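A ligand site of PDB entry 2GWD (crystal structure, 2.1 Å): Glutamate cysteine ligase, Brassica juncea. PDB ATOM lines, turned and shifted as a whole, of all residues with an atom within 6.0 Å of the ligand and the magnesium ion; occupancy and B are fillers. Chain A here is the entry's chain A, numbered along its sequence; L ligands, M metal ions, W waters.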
ATOM      1  N   GLU A  40     -27.722  -5.178   3.123  1.00  0.00           N
ATOM      2  CA  GLU A  40     -26.935  -3.953   3.033  1.00  0.00           C
ATOM      3  C   GLU A  40     -27.791  -2.848   2.450  1.00  0.00           C
ATOM      4  O   GLU A  40     -28.549  -3.077   1.493  1.00  0.00           O
ATOM      5  CB  GLU A  40     -25.734  -4.082   2.116  1.00  0.00           C
ATOM      6  CG  GLU A  40     -24.825  -5.250   2.331  1.00  0.00           C
ATOM      7  CD  GLU A  40     -23.610  -5.221   1.389  1.00  0.00           C
ATOM      8  OE1 GLU A  40     -23.475  -4.300   0.553  1.00  0.00           O
ATOM      9  OE2 GLU A  40     -22.810  -6.184   1.461  1.00  0.00           O
ATOM     10  N   GLU A  42     -27.643   1.719   1.702  1.00  0.00           N
ATOM     11  CA  GLU A  42     -26.869   2.941   1.615  1.00  0.00           C
ATOM     12  C   GLU A  42     -27.848   4.119   1.693  1.00  0.00           C
ATOM     13  O   GLU A  42     -28.981   4.021   1.184  1.00  0.00           O
ATOM     14  CB  GLU A  42     -26.112   2.992   0.268  1.00  0.00           C
ATOM     15  CG  GLU A  42     -25.103   1.885   0.095  1.00  0.00           C
ATOM     16  CD  GLU A  42     -24.727   1.605  -1.345  1.00  0.00           C
ATOM     17  OE1 GLU A  42     -25.412   2.098  -2.252  1.00  0.00           O
ATOM     18  OE2 GLU A  42     -23.715   0.870  -1.558  1.00  0.00           O
ATOM     19  N   SER A  92     -19.908   1.516   6.670  1.00  0.00           N
ATOM     20  CA  SER A  92     -18.887   1.918   5.713  1.00  0.00           C
ATOM     21  C   SER A  92     -19.370   3.084   4.842  1.00  0.00           C
ATOM     22  O   SER A  92     -20.501   3.561   4.988  1.00  0.00           O
ATOM     23  CB  SER A  92     -18.494   0.711   4.860  1.00  0.00           C
ATOM     24  OG  SER A  92     -19.502   0.407   3.933  1.00  0.00           O
ATOM     25  N   GLU A  94     -19.580   4.708   0.915  1.00  0.00           N
ATOM     26  CA  GLU A  94     -19.444   4.695  -0.532  1.00  0.00           C
ATOM     27  C   GLU A  94     -18.733   5.999  -0.982  1.00  0.00           C
ATOM     28  O   GLU A  94     -18.546   6.901  -0.173  1.00  0.00           O
ATOM     29  CB  GLU A  94     -20.797   4.481  -1.176  1.00  0.00           C
ATOM     30  CG  GLU A  94     -21.400   3.092  -0.927  1.00  0.00           C
ATOM     31  CD  GLU A  94     -20.596   1.956  -1.568  1.00  0.00           C
ATOM     32  OE1 GLU A  94     -19.808   2.213  -2.502  1.00  0.00           O
ATOM     33  OE2 GLU A  94     -20.754   0.800  -1.144  1.00  0.00           O
ATOM     34  N   GLN A  98     -22.039   8.157   0.763  1.00  0.00           N
ATOM     35  CA  GLN A  98     -23.256   7.395   1.037  1.00  0.00           C
ATOM     36  C   GLN A  98     -22.939   6.485   2.217  1.00  0.00           C
ATOM     37  O   GLN A  98     -21.870   5.866   2.282  1.00  0.00           O
ATOM     38  CB  GLN A  98     -23.758   6.597  -0.169  1.00  0.00           C
ATOM     39  CG  GLN A  98     -23.912   7.404  -1.476  1.00  0.00           C
ATOM     40  CD  GLN A  98     -22.683   7.287  -2.349  1.00  0.00           C
ATOM     41  OE1 GLN A  98     -21.574   7.621  -1.921  1.00  0.00           O
ATOM     42  NE2 GLN A  98     -22.878   6.797  -3.600  1.00  0.00           N
ATOM     43  N   GLU A 100     -23.376   3.527   4.648  1.00  0.00           N
ATOM     44  CA  GLU A 100     -23.797   2.139   4.512  1.00  0.00           C
ATOM     45  C   GLU A 100     -23.758   1.331   5.802  1.00  0.00           C
ATOM     46  O   GLU A 100     -22.796   1.406   6.545  1.00  0.00           O
ATOM     47  CB  GLU A 100     -22.870   1.430   3.543  1.00  0.00           C
ATOM     48  CG  GLU A 100     -23.180  -0.054   3.388  1.00  0.00           C
ATOM     49  CD  GLU A 100     -22.429  -0.672   2.246  1.00  0.00           C
ATOM     50  OE1 GLU A 100     -22.494  -0.080   1.151  1.00  0.00           O
ATOM     51  OE2 GLU A 100     -21.759  -1.710   2.431  1.00  0.00           O
ATOM     52  N   GLY A 138     -32.725   6.239  -4.579  1.00  0.00           N
ATOM     53  CA  GLY A 138     -31.766   5.562  -5.427  1.00  0.00           C
ATOM     54  C   GLY A 138     -30.720   6.438  -6.073  1.00  0.00           C
ATOM     55  O   GLY A 138     -29.654   5.951  -6.446  1.00  0.00           O
ATOM     56  N   MET A 173     -22.547   6.497 -10.654  1.00  0.00           N
ATOM     57  CA  MET A 173     -22.700   5.316  -9.865  1.00  0.00           C
ATOM     58  C   MET A 173     -21.990   5.538  -8.530  1.00  0.00           C
ATOM     59  O   MET A 173     -22.599   5.416  -7.464  1.00  0.00           O
ATOM     60  CB  MET A 173     -22.127   4.088 -10.585  1.00  0.00           C
ATOM     61  CG  MET A 173     -22.351   2.780  -9.831  1.00  0.00           C
ATOM     62  SD  MET A 173     -21.074   2.525  -8.564  1.00  0.00           S
ATOM     63  CE  MET A 173     -19.725   1.977  -9.597  1.00  0.00           C
ATOM     64  N   MET A 174     -20.727   5.926  -8.598  1.00  0.00           N
ATOM     65  CA  MET A 174     -19.904   6.030  -7.402  1.00  0.00           C
ATOM     66  C   MET A 174     -20.386   7.099  -6.428  1.00  0.00           C
ATOM     67  O   MET A 174     -20.476   6.851  -5.226  1.00  0.00           O
ATOM     68  CB  MET A 174     -18.463   6.349  -7.815  1.00  0.00           C
ATOM     69  CG  MET A 174     -17.789   5.206  -8.485  1.00  0.00           C
ATOM     70  SD  MET A 174     -16.074   5.586  -8.829  1.00  0.00           S
ATOM     71  CE  MET A 174     -15.377   5.670  -7.175  1.00  0.00           C
ATOM     72  N   THR A 177     -25.474   7.350  -6.329  1.00  0.00           N
ATOM     73  CA  THR A 177     -26.477   6.290  -6.178  1.00  0.00           C
ATOM     74  C   THR A 177     -26.458   5.630  -4.805  1.00  0.00           C
ATOM     75  O   THR A 177     -25.433   5.624  -4.111  1.00  0.00           O
ATOM     76  CB  THR A 177     -26.368   5.170  -7.265  1.00  0.00           C
ATOM     77  OG1 THR A 177     -25.175   4.397  -7.103  1.00  0.00           O
ATOM     78  CG2 THR A 177     -26.427   5.745  -8.648  1.00  0.00           C
ATOM     79  N   CYS A 178     -27.595   5.090  -4.409  1.00  0.00           N
ATOM     80  CA  CYS A 178     -27.751   4.294  -3.190  1.00  0.00           C
ATOM     81  C   CYS A 178     -28.576   3.051  -3.491  1.00  0.00           C
ATOM     82  O   CYS A 178     -29.615   3.163  -4.125  1.00  0.00           O
ATOM     83  CB  CYS A 178     -28.507   5.080  -2.123  1.00  0.00           C
ATOM     84  SG  CYS A 178     -27.545   6.172  -1.100  1.00  0.00           S
ATOM     85  N   THR A 179     -28.126   1.901  -2.993  1.00  0.00           N
ATOM     86  CA  THR A 179     -28.827   0.633  -3.151  1.00  0.00           C
ATOM     87  C   THR A 179     -29.310   0.083  -1.805  1.00  0.00           C
ATOM     88  O   THR A 179     -28.829   0.477  -0.732  1.00  0.00           O
ATOM     89  CB  THR A 179     -27.921  -0.477  -3.806  1.00  0.00           C
ATOM     90  OG1 THR A 179     -28.709  -1.631  -4.147  1.00  0.00           O
ATOM     91  CG2 THR A 179     -26.859  -0.939  -2.872  1.00  0.00           C
ATOM     92  N   GLN A 181     -29.519  -3.984  -0.887  1.00  0.00           N
ATOM     93  CA  GLN A 181     -29.306  -5.339  -1.378  1.00  0.00           C
ATOM     94  C   GLN A 181     -29.401  -6.390  -0.284  1.00  0.00           C
ATOM     95  O   GLN A 181     -29.439  -6.103   0.925  1.00  0.00           O
ATOM     96  CB  GLN A 181     -27.964  -5.462  -2.102  1.00  0.00           C
ATOM     97  CG  GLN A 181     -26.746  -5.368  -1.245  1.00  0.00           C
ATOM     98  CD  GLN A 181     -25.489  -5.485  -2.086  1.00  0.00           C
ATOM     99  OE1 GLN A 181     -25.104  -4.546  -2.799  1.00  0.00           O
ATOM    100  NE2 GLN A 181     -24.835  -6.644  -2.019  1.00  0.00           N
ATOM    101  N   ARG A 227     -30.833   5.310 -11.234  1.00  0.00           N
ATOM    102  CA  ARG A 227     -29.797   4.474 -10.639  1.00  0.00           C
ATOM    103  C   ARG A 227     -29.544   3.230 -11.493  1.00  0.00           C
ATOM    104  O   ARG A 227     -28.398   2.964 -11.853  1.00  0.00           O
ATOM    105  CB  ARG A 227     -30.167   4.068  -9.217  1.00  0.00           C
ATOM    106  CG  ARG A 227     -29.215   3.076  -8.608  1.00  0.00           C
ATOM    107  CD  ARG A 227     -29.677   2.533  -7.259  1.00  0.00           C
ATOM    108  NE  ARG A 227     -28.999   1.273  -7.015  1.00  0.00           N
ATOM    109  CZ  ARG A 227     -29.412   0.095  -7.480  1.00  0.00           C
ATOM    110  NH1 ARG A 227     -30.575  -0.015  -8.119  1.00  0.00           N
ATOM    111  NH2 ARG A 227     -28.686  -0.980  -7.285  1.00  0.00           N
ATOM    112  N   TRP A 231     -26.138   2.050 -14.141  1.00  0.00           N
ATOM    113  CA  TRP A 231     -25.405   0.795 -14.211  1.00  0.00           C
ATOM    114  C   TRP A 231     -25.296   0.196 -15.605  1.00  0.00           C
ATOM    115  O   TRP A 231     -24.621  -0.824 -15.778  1.00  0.00           O
ATOM    116  CB  TRP A 231     -26.020  -0.213 -13.248  1.00  0.00           C
ATOM    117  CG  TRP A 231     -25.609  -0.033 -11.828  1.00  0.00           C
ATOM    118  CD1 TRP A 231     -26.392   0.407 -10.808  1.00  0.00           C
ATOM    119  CD2 TRP A 231     -24.336  -0.339 -11.270  1.00  0.00           C
ATOM    120  NE1 TRP A 231     -25.681   0.405  -9.636  1.00  0.00           N
ATOM    121  CE2 TRP A 231     -24.408  -0.044  -9.889  1.00  0.00           C
ATOM    122  CE3 TRP A 231     -23.137  -0.826 -11.795  1.00  0.00           C
ATOM    123  CZ2 TRP A 231     -23.327  -0.227  -9.027  1.00  0.00           C
ATOM    124  CZ3 TRP A 231     -22.069  -1.003 -10.953  1.00  0.00           C
ATOM    125  CH2 TRP A 231     -22.162  -0.714  -9.575  1.00  0.00           C
ATOM    126  N   THR A 307     -15.105  -8.400  -5.566  1.00  0.00           N
ATOM    127  CA  THR A 307     -15.935  -7.323  -5.020  1.00  0.00           C
ATOM    128  C   THR A 307     -15.824  -6.071  -5.929  1.00  0.00           C
ATOM    129  O   THR A 307     -16.495  -5.055  -5.704  1.00  0.00           O
ATOM    130  CB  THR A 307     -15.526  -7.053  -3.534  1.00  0.00           C
ATOM    131  OG1 THR A 307     -15.616  -8.296  -2.804  1.00  0.00           O
ATOM    132  CG2 THR A 307     -16.402  -6.035  -2.842  1.00  0.00           C
ATOM    133  N   PHE A 310     -19.636  -6.035 -10.736  1.00  0.00           N
ATOM    134  CA  PHE A 310     -20.906  -5.441 -10.396  1.00  0.00           C
ATOM    135  C   PHE A 310     -22.073  -5.850 -11.317  1.00  0.00           C
ATOM    136  O   PHE A 310     -22.738  -4.991 -11.853  1.00  0.00           O
ATOM    137  CB  PHE A 310     -20.778  -3.918 -10.398  1.00  0.00           C
ATOM    138  CG  PHE A 310     -19.637  -3.358  -9.566  1.00  0.00           C
ATOM    139  CD1 PHE A 310     -19.593  -3.552  -8.184  1.00  0.00           C
ATOM    140  CD2 PHE A 310     -18.668  -2.550 -10.160  1.00  0.00           C
ATOM    141  CE1 PHE A 310     -18.577  -2.990  -7.412  1.00  0.00           C
ATOM    142  CE2 PHE A 310     -17.637  -1.996  -9.403  1.00  0.00           C
ATOM    143  CZ  PHE A 310     -17.588  -2.210  -8.020  1.00  0.00           C
ATOM    144  N   ARG A 314     -24.478 -10.818  -8.222  1.00  0.00           N
ATOM    145  CA  ARG A 314     -23.075 -11.077  -8.068  1.00  0.00           C
ATOM    146  C   ARG A 314     -22.867 -12.369  -7.286  1.00  0.00           C
ATOM    147  O   ARG A 314     -23.591 -12.639  -6.346  1.00  0.00           O
ATOM    148  CB  ARG A 314     -22.407  -9.908  -7.347  1.00  0.00           C
ATOM    149  CG  ARG A 314     -20.962 -10.134  -6.980  1.00  0.00           C
ATOM    150  CD  ARG A 314     -20.598  -9.271  -5.789  1.00  0.00           C
ATOM    151  NE  ARG A 314     -20.041  -8.048  -6.217  1.00  0.00           N
ATOM    152  CZ  ARG A 314     -19.703  -7.044  -5.418  1.00  0.00           C
ATOM    153  NH1 ARG A 314     -19.929  -7.048  -4.107  1.00  0.00           N
ATOM    154  NH2 ARG A 314     -19.121  -6.006  -5.990  1.00  0.00           N
ATOM    155  N   ARG A 322     -28.674  -7.270  -6.610  1.00  0.00           N
ATOM    156  CA  ARG A 322     -28.017  -5.966  -6.697  1.00  0.00           C
ATOM    157  C   ARG A 322     -28.888  -4.953  -7.431  1.00  0.00           C
ATOM    158  O   ARG A 322     -28.377  -4.010  -8.034  1.00  0.00           O
ATOM    159  CB  ARG A 322     -26.652  -6.101  -7.394  1.00  0.00           C
ATOM    160  CG  ARG A 322     -25.601  -6.816  -6.573  1.00  0.00           C
ATOM    161  CD  ARG A 322     -24.230  -6.840  -7.208  1.00  0.00           C
ATOM    162  NE  ARG A 322     -23.798  -5.505  -7.638  1.00  0.00           N
ATOM    163  CZ  ARG A 322     -23.090  -4.675  -6.882  1.00  0.00           C
ATOM    164  NH1 ARG A 322     -22.732  -5.028  -5.653  1.00  0.00           N
ATOM    165  NH2 ARG A 322     -22.749  -3.484  -7.349  1.00  0.00           N
ATOM    166  N   ALA A 324     -31.783  -3.071  -6.763  1.00  0.00           N
ATOM    167  CA  ALA A 324     -32.873  -2.309  -6.165  1.00  0.00           C
ATOM    168  C   ALA A 324     -32.394  -0.952  -5.665  1.00  0.00           C
ATOM    169  O   ALA A 324     -31.300  -0.831  -5.132  1.00  0.00           O
ATOM    170  CB  ALA A 324     -33.516  -3.100  -5.034  1.00  0.00           C
HETATM  171  N1  LIG L   1     -24.207   2.511  -4.536  1.00  0.00           N
HETATM  172  C1  LIG L   1     -24.385   1.493  -5.591  1.00  0.00           C
HETATM  173  C2  LIG L   1     -25.854   1.459  -6.104  1.00  0.00           C
HETATM  174  O1  LIG L   1     -26.199   0.458  -6.750  1.00  0.00           O
HETATM  175  C3  LIG L   1     -23.921   0.119  -5.078  1.00  0.00           C
HETATM  176  C4  LIG L   1     -22.436   0.233  -4.644  1.00  0.00           C
HETATM  177  C5  LIG L   1     -21.865  -1.090  -4.127  1.00  0.00           C
HETATM  178  O2  LIG L   1     -21.183  -1.767  -4.945  1.00  0.00           O
HETATM  179  O3  LIG L   1     -22.113  -1.381  -2.915  1.00  0.00           O
HETATM  180  O4  LIG L   1     -26.607   2.404  -5.856  1.00  0.00           O
HETATM  181 MG    MG M   1     -22.317  -0.476  -0.906  1.00  0.00          MG
HETATM  182  O   HOH W   1     -19.510  -3.625  -4.127  1.00  0.00           O
HETATM  183  O   HOH W   2     -24.109  -1.849  -0.601  1.00  0.00           O
HETATM  184  O   HOH W   3     -21.028  -2.335  -0.408  1.00  0.00           O
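A nitrogen (N1) of the ligand is in hydrogen-bond range of the backbone carbonyl oxygen (O) of Thr 177 (3.4 Å).
The side-chain hydroxyl (OG1) of Thr 177 is in hydrogen-bond range of an oxygen (O4) of the ligand, 2.8 Å away.
The guanidinium group (NE) of Arg 227 is in salt-bridge range of an oxygen (O4) of the ligand, at 2.9 Å.
NE1 of Trp 231 lies within hydrogen-bond range of O1 of the ligand, 2.9 Å away.
An oxygen (O4) of the ligand sits close to the backbone NH (N) of Cys 178, at 3.2 Å.
N of Thr 179 lies within hydrogen-bond range of O4 of the ligand, at 3.3 Å.
An oxygen (O2) of the ligand lies within salt-bridge range of the guanidinium group (NH2) of Arg 322.
The backbone carbonyl oxygen (O) of Glu 42 sits at hydrogen-bond distance from the side-chain sulfur (SG) of Cys 178, at 3.5 Å.
The side-chain carboxylate of Glu 42 lies within hydrogen-bond range of the backbone NH of Thr 179 (2.8 Å).
O of Glu 100 lies within hydrogen-bond range of N of Ser 92, 2.9 Å away.
The backbone carbonyl oxygen (O) of Met 173 lies within hydrogen-bond range of the side-chain hydroxyl (OG1) of Thr 177, 2.8 Å away.
NH2 of Arg 227 sits at hydrogen-bond distance from OG1 of Thr 179, 3.2 Å away.
NH2 of Arg 227 lies within hydrogen-bond range of O of Arg 322 (3.1 Å).
The backbone carbonyl oxygen of Ala 324 lies close to the guanidinium group of Arg 227.
The side-chain hydroxyl of Thr 179 sits at hydrogen-bond distance from the backbone carbonyl oxygen of Ala 324 (2.9 Å).
Phe 310 touches the ligand.
Hydrophobic or aromatic side chains that line the ligand: Trp 231 and Phe 310.
The nearest printed residue that does not touch the ligand is Glu 100 (4.3 Å).
The nearest printed residue that does not touch the magnesium ion is Glu 40 (4.3 Å).
The magnesium ion is bound by OE2 of Glu 94 (2.0 Å), OE2 of Glu 42 (2.0 Å), OE1 of Glu 100 (2.1 Å), O3 of the ligand (2.2 Å), water W2 (2.3 Å) and water W3 (2.3 Å).
The magnesium ion has six donor atoms within binding distance.
Water W3 bridges the side-chain carboxylate of Glu 100 (3.0 Å) and the side-chain carboxylate of Glu 40 (3.3 Å).
Water W1 lies within hydrogen-bond range of O2 of the ligand (2.6 Å) and NH2 of Arg 314 (3.0 Å).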
